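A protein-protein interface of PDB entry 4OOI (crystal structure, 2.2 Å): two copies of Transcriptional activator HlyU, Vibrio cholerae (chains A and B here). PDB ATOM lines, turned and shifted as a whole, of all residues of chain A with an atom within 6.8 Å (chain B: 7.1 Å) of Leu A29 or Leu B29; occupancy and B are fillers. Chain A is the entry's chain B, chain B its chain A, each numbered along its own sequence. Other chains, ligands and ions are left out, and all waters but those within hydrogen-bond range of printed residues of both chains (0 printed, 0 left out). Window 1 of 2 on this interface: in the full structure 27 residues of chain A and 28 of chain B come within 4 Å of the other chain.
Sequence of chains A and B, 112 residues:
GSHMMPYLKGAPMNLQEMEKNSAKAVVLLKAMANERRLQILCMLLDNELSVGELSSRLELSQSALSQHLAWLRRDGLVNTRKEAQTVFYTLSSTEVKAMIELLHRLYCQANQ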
ATOM      1  N   SER A  22     -12.915  15.797  20.990  1.00  0.00           N
ATOM      2  CA  SER A  22     -12.426  14.435  20.840  1.00  0.00           C
ATOM      3  C   SER A  22     -13.456  13.446  21.356  1.00  0.00           C
ATOM      4  O   SER A  22     -13.449  12.287  20.965  1.00  0.00           O
ATOM      5  CB  SER A  22     -11.102  14.236  21.577  1.00  0.00           C
ATOM      6  OG  SER A  22     -11.284  14.335  22.978  1.00  0.00           O
ATOM      7  N   LYS A  24     -16.781  13.728  20.790  1.00  0.00           N
ATOM      8  CA  LYS A  24     -17.618  13.537  19.610  1.00  0.00           C
ATOM      9  C   LYS A  24     -16.895  12.692  18.570  1.00  0.00           C
ATOM     10  O   LYS A  24     -17.449  11.720  18.038  1.00  0.00           O
ATOM     11  CB  LYS A  24     -17.987  14.887  18.991  1.00  0.00           C
ATOM     12  CG  LYS A  24     -18.622  15.883  19.948  1.00  0.00           C
ATOM     13  CD  LYS A  24     -19.013  17.160  19.220  1.00  0.00           C
ATOM     14  CE  LYS A  24     -19.575  18.202  20.174  1.00  0.00           C
ATOM     15  NZ  LYS A  24     -18.569  18.636  21.184  1.00  0.00           N
ATOM     16  N   ALA A  25     -15.651  13.074  18.286  1.00  0.00           N
ATOM     17  CA  ALA A  25     -14.830  12.371  17.304  1.00  0.00           C
ATOM     18  C   ALA A  25     -14.699  10.891  17.647  1.00  0.00           C
ATOM     19  O   ALA A  25     -14.698  10.036  16.762  1.00  0.00           O
ATOM     20  CB  ALA A  25     -13.457  13.018  17.204  1.00  0.00           C
ATOM     21  N   VAL A  26     -14.597  10.599  18.939  1.00  0.00           N
ATOM     22  CA  VAL A  26     -14.485   9.226  19.416  1.00  0.00           C
ATOM     23  C   VAL A  26     -15.826   8.501  19.327  1.00  0.00           C
ATOM     24  O   VAL A  26     -15.866   7.297  19.097  1.00  0.00           O
ATOM     25  CB  VAL A  26     -13.886   9.163  20.846  1.00  0.00           C
ATOM     26  CG1 VAL A  26     -14.197   7.841  21.529  1.00  0.00           C
ATOM     27  CG2 VAL A  26     -12.389   9.379  20.782  1.00  0.00           C
ATOM     28  N   VAL A  27     -16.926   9.231  19.486  1.00  0.00           N
ATOM     29  CA  VAL A  27     -18.237   8.638  19.240  1.00  0.00           C
ATOM     30  C   VAL A  27     -18.316   8.164  17.787  1.00  0.00           C
ATOM     31  O   VAL A  27     -18.692   7.014  17.508  1.00  0.00           O
ATOM     32  CB  VAL A  27     -19.385   9.623  19.535  1.00  0.00           C
ATOM     33  CG1 VAL A  27     -20.710   9.063  19.041  1.00  0.00           C
ATOM     34  CG2 VAL A  27     -19.454   9.926  21.023  1.00  0.00           C
ATOM     35  N   LEU A  28     -17.930   9.046  16.867  1.00  0.00           N
ATOM     36  CA  LEU A  28     -17.900   8.686  15.450  1.00  0.00           C
ATOM     37  C   LEU A  28     -16.987   7.493  15.178  1.00  0.00           C
ATOM     38  O   LEU A  28     -17.381   6.550  14.496  1.00  0.00           O
ATOM     39  CB  LEU A  28     -17.468   9.871  14.583  1.00  0.00           C
ATOM     40  CG  LEU A  28     -18.447  11.031  14.390  1.00  0.00           C
ATOM     41  CD1 LEU A  28     -18.247  11.652  13.016  1.00  0.00           C
ATOM     42  CD2 LEU A  28     -19.888  10.587  14.577  1.00  0.00           C
ATOM     43  N   LEU A  29     -15.772   7.542  15.717  1.00  0.00           N
ATOM     44  CA  LEU A  29     -14.788   6.483  15.496  1.00  0.00           C
ATOM     45  C   LEU A  29     -15.249   5.131  16.036  1.00  0.00           C
ATOM     46  O   LEU A  29     -15.074   4.102  15.384  1.00  0.00           O
ATOM     47  CB  LEU A  29     -13.439   6.869  16.106  1.00  0.00           C
ATOM     48  CG  LEU A  29     -12.695   7.989  15.380  1.00  0.00           C
ATOM     49  CD1 LEU A  29     -11.512   8.474  16.198  1.00  0.00           C
ATOM     50  CD2 LEU A  29     -12.242   7.515  14.010  1.00  0.00           C
ATOM     51  N   LYS A  30     -15.833   5.142  17.230  1.00  0.00           N
ATOM     52  CA  LYS A  30     -16.398   3.942  17.834  1.00  0.00           C
ATOM     53  C   LYS A  30     -17.493   3.389  16.940  1.00  0.00           C
ATOM     54  O   LYS A  30     -17.585   2.177  16.732  1.00  0.00           O
ATOM     55  CB  LYS A  30     -16.978   4.252  19.217  1.00  0.00           C
ATOM     56  CG  LYS A  30     -15.953   4.339  20.336  1.00  0.00           C
ATOM     57  CD  LYS A  30     -16.593   4.871  21.611  1.00  0.00           C
ATOM     58  CE  LYS A  30     -15.671   4.722  22.811  1.00  0.00           C
ATOM     59  NZ  LYS A  30     -15.512   3.298  23.210  1.00  0.00           N
ATOM     60  N   ALA A  31     -18.323   4.282  16.410  1.00  0.00           N
ATOM     61  CA  ALA A  31     -19.382   3.865  15.499  1.00  0.00           C
ATOM     62  C   ALA A  31     -18.817   3.272  14.208  1.00  0.00           C
ATOM     63  O   ALA A  31     -19.425   2.388  13.602  1.00  0.00           O
ATOM     64  CB  ALA A  31     -20.306   5.027  15.196  1.00  0.00           C
ATOM     65  N   MET A  32     -17.647   3.751  13.798  1.00  0.00           N
ATOM     66  CA  MET A  32     -17.013   3.272  12.573  1.00  0.00           C
ATOM     67  C   MET A  32     -16.099   2.077  12.822  1.00  0.00           C
ATOM     68  O   MET A  32     -15.766   1.342  11.894  1.00  0.00           O
ATOM     69  CB  MET A  32     -16.218   4.397  11.902  1.00  0.00           C
ATOM     70  CG  MET A  32     -17.062   5.571  11.442  1.00  0.00           C
ATOM     71  SD  MET A  32     -16.087   6.818  10.580  1.00  0.00           S
ATOM     72  CE  MET A  32     -17.308   8.109  10.356  1.00  0.00           C
ATOM     73  N   ALA A  33     -15.703   1.881  14.076  1.00  0.00           N
ATOM     74  CA  ALA A  33     -14.773   0.809  14.430  1.00  0.00           C
ATOM     75  C   ALA A  33     -15.430  -0.568  14.406  1.00  0.00           C
ATOM     76  O   ALA A  33     -15.356  -1.321  15.376  1.00  0.00           O
ATOM     77  CB  ALA A  33     -14.145   1.074  15.791  1.00  0.00           C
ATOM     78  N   ASN A  34     -16.072  -0.887  13.288  1.00  0.00           N
ATOM     79  CA  ASN A  34     -16.700  -2.185  13.094  1.00  0.00           C
ATOM     80  C   ASN A  34     -16.790  -2.488  11.608  1.00  0.00           C
ATOM     81  O   ASN A  34     -17.215  -1.638  10.826  1.00  0.00           O
ATOM     82  CB  ASN A  34     -18.093  -2.210  13.720  1.00  0.00           C
ATOM     83  CG  ASN A  34     -18.760  -3.565  13.603  1.00  0.00           C
ATOM     84  OD1 ASN A  34     -19.369  -3.885  12.582  1.00  0.00           O
ATOM     85  ND2 ASN A  34     -18.652  -4.371  14.654  1.00  0.00           N
ATOM     86  N   ARG A  37     -20.427  -2.239  10.088  1.00  0.00           N
ATOM     87  CA  ARG A  37     -20.867  -0.848  10.134  1.00  0.00           C
ATOM     88  C   ARG A  37     -20.099   0.007   9.131  1.00  0.00           C
ATOM     89  O   ARG A  37     -20.669   0.886   8.487  1.00  0.00           O
ATOM     90  CB  ARG A  37     -20.722  -0.277  11.545  1.00  0.00           C
ATOM     91  CG  ARG A  37     -21.591  -0.972  12.581  1.00  0.00           C
ATOM     92  CD  ARG A  37     -21.888  -0.060  13.761  1.00  0.00           C
ATOM     93  NE  ARG A  37     -20.689   0.290  14.517  1.00  0.00           N
ATOM     94  CZ  ARG A  37     -20.274  -0.361  15.600  1.00  0.00           C
ATOM     95  NH1 ARG A  37     -20.958  -1.402  16.053  1.00  0.00           N
ATOM     96  NH2 ARG A  37     -19.172   0.027  16.228  1.00  0.00           N
ATOM     97  N   LEU A  38     -18.805  -0.267   8.998  1.00  0.00           N
ATOM     98  CA  LEU A  38     -17.968   0.448   8.043  1.00  0.00           C
ATOM     99  C   LEU A  38     -18.389   0.141   6.611  1.00  0.00           C
ATOM    100  O   LEU A  38     -18.351   1.016   5.746  1.00  0.00           O
ATOM    101  CB  LEU A  38     -16.497   0.087   8.242  1.00  0.00           C
ATOM    102  CG  LEU A  38     -15.503   0.822   7.344  1.00  0.00           C
ATOM    103  CD1 LEU A  38     -15.587   2.322   7.573  1.00  0.00           C
ATOM    104  CD2 LEU A  38     -14.099   0.315   7.599  1.00  0.00           C
ATOM    105  N   LEU A  77     -24.922   8.901  12.652  1.00  0.00           N
ATOM    106  CA  LEU A  77     -24.063   8.770  11.480  1.00  0.00           C
ATOM    107  C   LEU A  77     -24.901   8.506  10.242  1.00  0.00           C
ATOM    108  O   LEU A  77     -24.384   8.468   9.125  1.00  0.00           O
ATOM    109  CB  LEU A  77     -23.047   7.642  11.659  1.00  0.00           C
ATOM    110  CG  LEU A  77     -21.822   7.938  12.526  1.00  0.00           C
ATOM    111  CD1 LEU A  77     -22.171   7.846  13.999  1.00  0.00           C
ATOM    112  CD2 LEU A  77     -20.678   7.003  12.175  1.00  0.00           C
ATOM    113  N   MET A  99     -15.054  11.642   6.545  1.00  0.00           N
ATOM    114  CA  MET A  99     -14.283  10.536   7.105  1.00  0.00           C
ATOM    115  C   MET A  99     -14.412   9.274   6.259  1.00  0.00           C
ATOM    116  O   MET A  99     -13.424   8.585   6.003  1.00  0.00           O
ATOM    117  CB  MET A  99     -14.718  10.255   8.546  1.00  0.00           C
ATOM    118  CG  MET A  99     -14.410  11.386   9.512  1.00  0.00           C
ATOM    119  SD  MET A  99     -14.982  11.052  11.188  1.00  0.00           S
ATOM    120  CE  MET A  99     -13.992   9.618  11.597  1.00  0.00           C
ATOM    121  N   ILE A 100     -15.634   8.981   5.824  1.00  0.00           N
ATOM    122  CA  ILE A 100     -15.892   7.823   4.976  1.00  0.00           C
ATOM    123  C   ILE A 100     -15.209   7.971   3.619  1.00  0.00           C
ATOM    124  O   ILE A 100     -14.628   7.017   3.103  1.00  0.00           O
ATOM    125  CB  ILE A 100     -17.405   7.577   4.792  1.00  0.00           C
ATOM    126  CG1 ILE A 100     -18.011   7.030   6.085  1.00  0.00           C
ATOM    127  CG2 ILE A 100     -17.664   6.607   3.651  1.00  0.00           C
ATOM    128  CD1 ILE A 100     -17.311   5.789   6.603  1.00  0.00           C
ATOM    129  N   LEU A 103     -11.545   7.336   4.176  1.00  0.00           N
ATOM    130  CA  LEU A 103     -11.324   5.905   4.371  1.00  0.00           C
ATOM    131  C   LEU A 103     -11.398   5.145   3.050  1.00  0.00           C
ATOM    132  O   LEU A 103     -10.652   4.189   2.828  1.00  0.00           O
ATOM    133  CB  LEU A 103     -12.340   5.334   5.364  1.00  0.00           C
ATOM    134  CG  LEU A 103     -12.151   5.725   6.832  1.00  0.00           C
ATOM    135  CD1 LEU A 103     -13.285   5.179   7.683  1.00  0.00           C
ATOM    136  CD2 LEU A 103     -10.809   5.231   7.345  1.00  0.00           C
ATOM    137  N   TYR A 107      -8.234   3.068   1.655  1.00  0.00           N
ATOM    138  CA  TYR A 107      -8.262   1.608   1.723  1.00  0.00           C
ATOM    139  C   TYR A 107      -8.914   0.903   0.533  1.00  0.00           C
ATOM    140  O   TYR A 107      -9.014  -0.323   0.522  1.00  0.00           O
ATOM    141  CB  TYR A 107      -8.928   1.149   3.025  1.00  0.00           C
ATOM    142  CG  TYR A 107      -8.124   1.472   4.263  1.00  0.00           C
ATOM    143  CD1 TYR A 107      -7.085   0.648   4.673  1.00  0.00           C
ATOM    144  CD2 TYR A 107      -8.404   2.602   5.022  1.00  0.00           C
ATOM    145  CE1 TYR A 107      -6.347   0.938   5.802  1.00  0.00           C
ATOM    146  CE2 TYR A 107      -7.670   2.899   6.155  1.00  0.00           C
ATOM    147  CZ  TYR A 107      -6.643   2.063   6.540  1.00  0.00           C
ATOM    148  OH  TYR A 107      -5.907   2.350   7.665  1.00  0.00           O
ATOM    149  N   SER B  22     -12.116  -3.159   4.829  1.00  0.00           N
ATOM    150  CA  SER B  22     -12.690  -2.803   6.120  1.00  0.00           C
ATOM    151  C   SER B  22     -11.963  -3.497   7.262  1.00  0.00           C
ATOM    152  O   SER B  22     -12.052  -3.061   8.397  1.00  0.00           O
ATOM    153  CB  SER B  22     -14.185  -3.130   6.185  1.00  0.00           C
ATOM    154  OG  SER B  22     -14.407  -4.528   6.122  1.00  0.00           O
ATOM    155  N   ALA B  23     -11.253  -4.581   6.971  1.00  0.00           N
ATOM    156  CA  ALA B  23     -10.487  -5.259   8.009  1.00  0.00           C
ATOM    157  C   ALA B  23      -9.338  -4.368   8.463  1.00  0.00           C
ATOM    158  O   ALA B  23      -9.232  -4.029   9.649  1.00  0.00           O
ATOM    159  CB  ALA B  23      -9.967  -6.601   7.518  1.00  0.00           C
ATOM    160  N   LYS B  24      -8.492  -3.970   7.516  1.00  0.00           N
ATOM    161  CA  LYS B  24      -7.380  -3.077   7.850  1.00  0.00           C
ATOM    162  C   LYS B  24      -7.876  -1.720   8.363  1.00  0.00           C
ATOM    163  O   LYS B  24      -7.370  -1.189   9.367  1.00  0.00           O
ATOM    164  CB  LYS B  24      -6.450  -2.891   6.649  1.00  0.00           C
ATOM    165  CG  LYS B  24      -5.620  -4.121   6.311  1.00  0.00           C
ATOM    166  CD  LYS B  24      -4.650  -3.839   5.176  1.00  0.00           C
ATOM    167  CE  LYS B  24      -3.745  -5.031   4.905  1.00  0.00           C
ATOM    168  NZ  LYS B  24      -2.800  -4.765   3.785  1.00  0.00           N
ATOM    169  N   ALA B  25      -8.875  -1.173   7.676  1.00  0.00           N
ATOM    170  CA  ALA B  25      -9.451   0.108   8.067  1.00  0.00           C
ATOM    171  C   ALA B  25      -9.991   0.073   9.495  1.00  0.00           C
ATOM    172  O   ALA B  25      -9.826   1.031  10.243  1.00  0.00           O
ATOM    173  CB  ALA B  25     -10.538   0.526   7.094  1.00  0.00           C
ATOM    174  N   VAL B  26     -10.622  -1.036   9.871  1.00  0.00           N
ATOM    175  CA  VAL B  26     -11.157  -1.189  11.223  1.00  0.00           C
ATOM    176  C   VAL B  26     -10.038  -1.431  12.235  1.00  0.00           C
ATOM    177  O   VAL B  26     -10.164  -1.060  13.397  1.00  0.00           O
ATOM    178  CB  VAL B  26     -12.267  -2.278  11.297  1.00  0.00           C
ATOM    179  CG1 VAL B  26     -12.466  -2.803  12.713  1.00  0.00           C
ATOM    180  CG2 VAL B  26     -13.574  -1.725  10.748  1.00  0.00           C
ATOM    181  N   VAL B  27      -8.934  -2.029  11.797  1.00  0.00           N
ATOM    182  CA  VAL B  27      -7.755  -2.077  12.659  1.00  0.00           C
ATOM    183  C   VAL B  27      -7.364  -0.648  13.033  1.00  0.00           C
ATOM    184  O   VAL B  27      -7.221  -0.312  14.222  1.00  0.00           O
ATOM    185  CB  VAL B  27      -6.563  -2.782  11.984  1.00  0.00           C
ATOM    186  CG1 VAL B  27      -5.294  -2.569  12.793  1.00  0.00           C
ATOM    187  CG2 VAL B  27      -6.849  -4.265  11.814  1.00  0.00           C
ATOM    188  N   LEU B  28      -7.228   0.199  12.014  1.00  0.00           N
ATOM    189  CA  LEU B  28      -6.897   1.608  12.240  1.00  0.00           C
ATOM    190  C   LEU B  28      -7.910   2.325  13.137  1.00  0.00           C
ATOM    191  O   LEU B  28      -7.536   2.988  14.105  1.00  0.00           O
ATOM    192  CB  LEU B  28      -6.776   2.356  10.911  1.00  0.00           C
ATOM    193  CG  LEU B  28      -6.535   3.863  11.056  1.00  0.00           C
ATOM    194  CD1 LEU B  28      -5.126   4.137  11.562  1.00  0.00           C
ATOM    195  CD2 LEU B  28      -6.801   4.602   9.752  1.00  0.00           C
ATOM    196  N   LEU B  29      -9.190   2.187  12.805  1.00  0.00           N
ATOM    197  CA  LEU B  29     -10.262   2.877  13.518  1.00  0.00           C
ATOM    198  C   LEU B  29     -10.363   2.444  14.978  1.00  0.00           C
ATOM    199  O   LEU B  29     -10.513   3.280  15.867  1.00  0.00           O
ATOM    200  CB  LEU B  29     -11.602   2.658  12.809  1.00  0.00           C
ATOM    201  CG  LEU B  29     -11.735   3.277  11.417  1.00  0.00           C
ATOM    202  CD1 LEU B  29     -13.028   2.836  10.749  1.00  0.00           C
ATOM    203  CD2 LEU B  29     -11.660   4.792  11.498  1.00  0.00           C
ATOM    204  N   LYS B  30     -10.294   1.137  15.211  1.00  0.00           N
ATOM    205  CA  LYS B  30     -10.283   0.590  16.563  1.00  0.00           C
ATOM    206  C   LYS B  30      -9.095   1.145  17.325  1.00  0.00           C
ATOM    207  O   LYS B  30      -9.204   1.470  18.508  1.00  0.00           O
ATOM    208  CB  LYS B  30     -10.207  -0.937  16.541  1.00  0.00           C
ATOM    209  CG  LYS B  30     -11.531  -1.635  16.288  1.00  0.00           C
ATOM    210  CD  LYS B  30     -11.363  -3.145  16.370  1.00  0.00           C
ATOM    211  CE  LYS B  30     -12.692  -3.863  16.221  1.00  0.00           C
ATOM    212  NZ  LYS B  30     -12.536  -5.336  16.359  1.00  0.00           N
ATOM    213  N   ALA B  31      -7.958   1.254  16.644  1.00  0.00           N
ATOM    214  CA  ALA B  31      -6.790   1.872  17.257  1.00  0.00           C
ATOM    215  C   ALA B  31      -7.045   3.347  17.578  1.00  0.00           C
ATOM    216  O   ALA B  31      -6.453   3.898  18.505  1.00  0.00           O
ATOM    217  CB  ALA B  31      -5.574   1.716  16.365  1.00  0.00           C
ATOM    218  N   MET B  32      -7.935   3.979  16.817  1.00  0.00           N
ATOM    219  CA  MET B  32      -8.247   5.392  17.028  1.00  0.00           C
ATOM    220  C   MET B  32      -9.525   5.623  17.833  1.00  0.00           C
ATOM    221  O   MET B  32      -9.779   6.738  18.287  1.00  0.00           O
ATOM    222  CB  MET B  32      -8.355   6.129  15.692  1.00  0.00           C
ATOM    223  CG  MET B  32      -7.092   6.103  14.850  1.00  0.00           C
ATOM    224  SD  MET B  32      -7.204   7.228  13.446  1.00  0.00           S
ATOM    225  CE  MET B  32      -8.755   6.711  12.720  1.00  0.00           C
ATOM    226  N   ALA B  33     -10.329   4.579  18.010  1.00  0.00           N
ATOM    227  CA  ALA B  33     -11.618   4.717  18.689  1.00  0.00           C
ATOM    228  C   ALA B  33     -11.487   4.810  20.207  1.00  0.00           C
ATOM    229  O   ALA B  33     -12.170   4.098  20.942  1.00  0.00           O
ATOM    230  CB  ALA B  33     -12.550   3.575  18.306  1.00  0.00           C
ATOM    231  N   ASN B  34     -10.612   5.697  20.667  1.00  0.00           N
ATOM    232  CA  ASN B  34     -10.397   5.911  22.093  1.00  0.00           C
ATOM    233  C   ASN B  34      -9.968   7.349  22.346  1.00  0.00           C
ATOM    234  O   ASN B  34      -9.112   7.874  21.638  1.00  0.00           O
ATOM    235  CB  ASN B  34      -9.338   4.944  22.621  1.00  0.00           C
ATOM    236  CG  ASN B  34      -9.103   5.091  24.110  1.00  0.00           C
ATOM    237  OD1 ASN B  34      -8.266   5.882  24.545  1.00  0.00           O
ATOM    238  ND2 ASN B  34      -9.838   4.320  24.903  1.00  0.00           N
ATOM    239  N   ARG B  37      -6.117   7.815  23.288  1.00  0.00           N
ATOM    240  CA  ARG B  37      -5.313   7.462  22.123  1.00  0.00           C
ATOM    241  C   ARG B  37      -5.484   8.474  20.993  1.00  0.00           C
ATOM    242  O   ARG B  37      -4.515   8.844  20.328  1.00  0.00           O
ATOM    243  CB  ARG B  37      -5.650   6.050  21.635  1.00  0.00           C
ATOM    244  CG  ARG B  37      -5.344   4.958  22.648  1.00  0.00           C
ATOM    245  CD  ARG B  37      -5.176   3.600  21.981  1.00  0.00           C
ATOM    246  NE  ARG B  37      -6.408   3.124  21.357  1.00  0.00           N
ATOM    247  CZ  ARG B  37      -7.303   2.351  21.963  1.00  0.00           C
ATOM    248  NH1 ARG B  37      -7.110   1.970  23.219  1.00  0.00           N
ATOM    249  NH2 ARG B  37      -8.395   1.965  21.318  1.00  0.00           N
ATOM    250  N   LEU B  38      -6.718   8.925  20.785  1.00  0.00           N
ATOM    251  CA  LEU B  38      -6.996   9.933  19.769  1.00  0.00           C
ATOM    252  C   LEU B  38      -6.301  11.245  20.107  1.00  0.00           C
ATOM    253  O   LEU B  38      -5.815  11.942  19.220  1.00  0.00           O
ATOM    254  CB  LEU B  38      -8.500  10.165  19.618  1.00  0.00           C
ATOM    255  CG  LEU B  38      -8.896  11.187  18.550  1.00  0.00           C
ATOM    256  CD1 LEU B  38      -8.457  10.710  17.173  1.00  0.00           C
ATOM    257  CD2 LEU B  38     -10.389  11.461  18.576  1.00  0.00           C
ATOM    258  N   LEU B  77       0.679   2.487  14.545  1.00  0.00           N
ATOM    259  CA  LEU B  77       0.204   3.845  14.298  1.00  0.00           C
ATOM    260  C   LEU B  77       1.257   4.880  14.674  1.00  0.00           C
ATOM    261  O   LEU B  77       1.216   6.016  14.202  1.00  0.00           O
ATOM    262  CB  LEU B  77      -1.097   4.123  15.054  1.00  0.00           C
ATOM    263  CG  LEU B  77      -2.406   3.745  14.357  1.00  0.00           C
ATOM    264  CD1 LEU B  77      -2.593   2.236  14.305  1.00  0.00           C
ATOM    265  CD2 LEU B  77      -3.588   4.417  15.041  1.00  0.00           C
ATOM    266  N   MET B  99      -5.978  10.710   8.442  1.00  0.00           N
ATOM    267  CA  MET B  99      -7.141  10.641   9.321  1.00  0.00           C
ATOM    268  C   MET B  99      -7.080  11.697  10.418  1.00  0.00           C
ATOM    269  O   MET B  99      -8.058  12.402  10.664  1.00  0.00           O
ATOM    270  CB  MET B  99      -7.276   9.248   9.937  1.00  0.00           C
ATOM    271  CG  MET B  99      -7.795   8.187   8.979  1.00  0.00           C
ATOM    272  SD  MET B  99      -9.470   8.530   8.396  1.00  0.00           S
ATOM    273  CE  MET B  99     -10.356   8.649   9.947  1.00  0.00           C
ATOM    274  N   ILE B 100      -5.926  11.809  11.069  1.00  0.00           N
ATOM    275  CA  ILE B 100      -5.741  12.792  12.133  1.00  0.00           C
ATOM    276  C   ILE B 100      -5.837  14.221  11.596  1.00  0.00           C
ATOM    277  O   ILE B 100      -6.380  15.105  12.259  1.00  0.00           O
ATOM    278  CB  ILE B 100      -4.413  12.571  12.893  1.00  0.00           C
ATOM    279  CG1 ILE B 100      -4.497  11.298  13.736  1.00  0.00           C
ATOM    280  CG2 ILE B 100      -4.097  13.746  13.797  1.00  0.00           C
ATOM    281  CD1 ILE B 100      -5.674  11.278  14.690  1.00  0.00           C
ATOM    282  N   LEU B 103      -9.641  14.807  11.007  1.00  0.00           N
ATOM    283  CA  LEU B 103     -10.285  14.967  12.307  1.00  0.00           C
ATOM    284  C   LEU B 103      -9.930  16.313  12.927  1.00  0.00           C
ATOM    285  O   LEU B 103     -10.746  16.924  13.617  1.00  0.00           O
ATOM    286  CB  LEU B 103      -9.873  13.835  13.250  1.00  0.00           C
ATOM    287  CG  LEU B 103     -10.385  12.440  12.894  1.00  0.00           C
ATOM    288  CD1 LEU B 103      -9.751  11.394  13.795  1.00  0.00           C
ATOM    289  CD2 LEU B 103     -11.900  12.393  12.998  1.00  0.00           C
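Ala A25 touches Leu B38 (CB to CD2, 3.7 Å).
Val A26 touches Asn B34 (CG2 to C, 3.5 Å).
CG2 of Val A26 touches CD2 of Leu B38, 3.6 Å away.
CD2 of Leu B29 touches CD2 of Leu A29, 3.8 Å away.
CG2 of Val B26 touches O of Met A32, 3.9 Å away.
Ala A33 touches Lys B30.
CB of Ala B25 touches CD2 of Leu A38, 3.6 Å away.
CD2 of Leu A38 touches CG2 of Val B26, 3.8 Å away.
Leu A103 touches Leu B29.
CB of Ala B25 touches CD2 of Tyr A107, at 3.6 Å.
The backbone NH of Arg A37 lies within hydrogen-bond range of the side-chain amide oxygen of Asn A34, at 3.2 Å.
N of Arg B37 sits at hydrogen-bond distance from OD1 of Asn B34 (3.2 Å).
The guanidinium group (NH2) of Arg B37 is in hydrogen-bond range of the backbone carbonyl oxygen (O) of Lys B30.
The guanidinium group of Arg A37 is in hydrogen-bond range of the backbone carbonyl oxygen of Lys A30 (2.7 Å).
Of the 19 printed residues of chain A, 12 touch a printed residue of chain B.
Printed residues of chain A that touch a printed residue of chain B: Ser A22, Ala A25, Val A26, Leu A29, Lys A30, Met A32, Ala A33, Asn A34, Leu A38, Met A99, Leu A103 and Tyr A107.
Hydrophobic or aromatic side chains of chain A that line the printed part of chain B: Ala A25, Val A26, Leu A29, Met A32, Ala A33, Leu A38, Met A99, Leu A103 and Tyr A107.
Along chain A the printed residues that touch a printed residue of chain B span positions 22 to 107.
Printed residues of chain B that touch a printed residue of chain A: Ser B22, Lys B24, Ala B25, Val B26, Leu B28, Leu B29, Lys B30, Met B32, Ala B33, Asn B34, Leu B38, Met B99 and Leu B103.
Among the printed residues, 23 pairs touch across the chains.
Among the printed residues, no Asp or Glu carboxylate lies within 4 Å of a Lys or Arg side-chain nitrogen of the other chain.
Val A26 touches Asn B34, and with the chains exchanged Asn A34 touches Val B26.
Val A26 touches Leu B38, and with the chains exchanged Leu A38 touches Val B26.
Leu B29 touches its own counterpart, Leu A29.
Ala B33 touches its own counterpart, Ala A33.
Leu A29 touches just these residues of chain B: Leu B29 (3.8 Å), Met B32 (3.2 Å), Ala B33 (3.8 Å) and Leu B38 (3.9 Å).
Of the printed residues of chain A, Leu B29 touches Leu A29, Met A32 and Leu A103.
Of the printed residues of chain B, Asn A34 touches Val B26.
Printed residues of chain A within 4 Å of Leu B38: Ser A22 (3.97 Å), Ala A25 (3.7 Å), Val A26 (3.6 Å) and Leu A29 (3.9 Å).
Printed residues of chain A within 4 Å of Leu B28: Tyr A107.
Leu A28 touches none of the printed residues of chain B.
The nearest residue of chain B that does not touch Leu A29 is Leu B103 (4.2 Å).
The nearest printed residue of chain A that does not touch Leu B29 is Ala A33 (4.01 Å).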
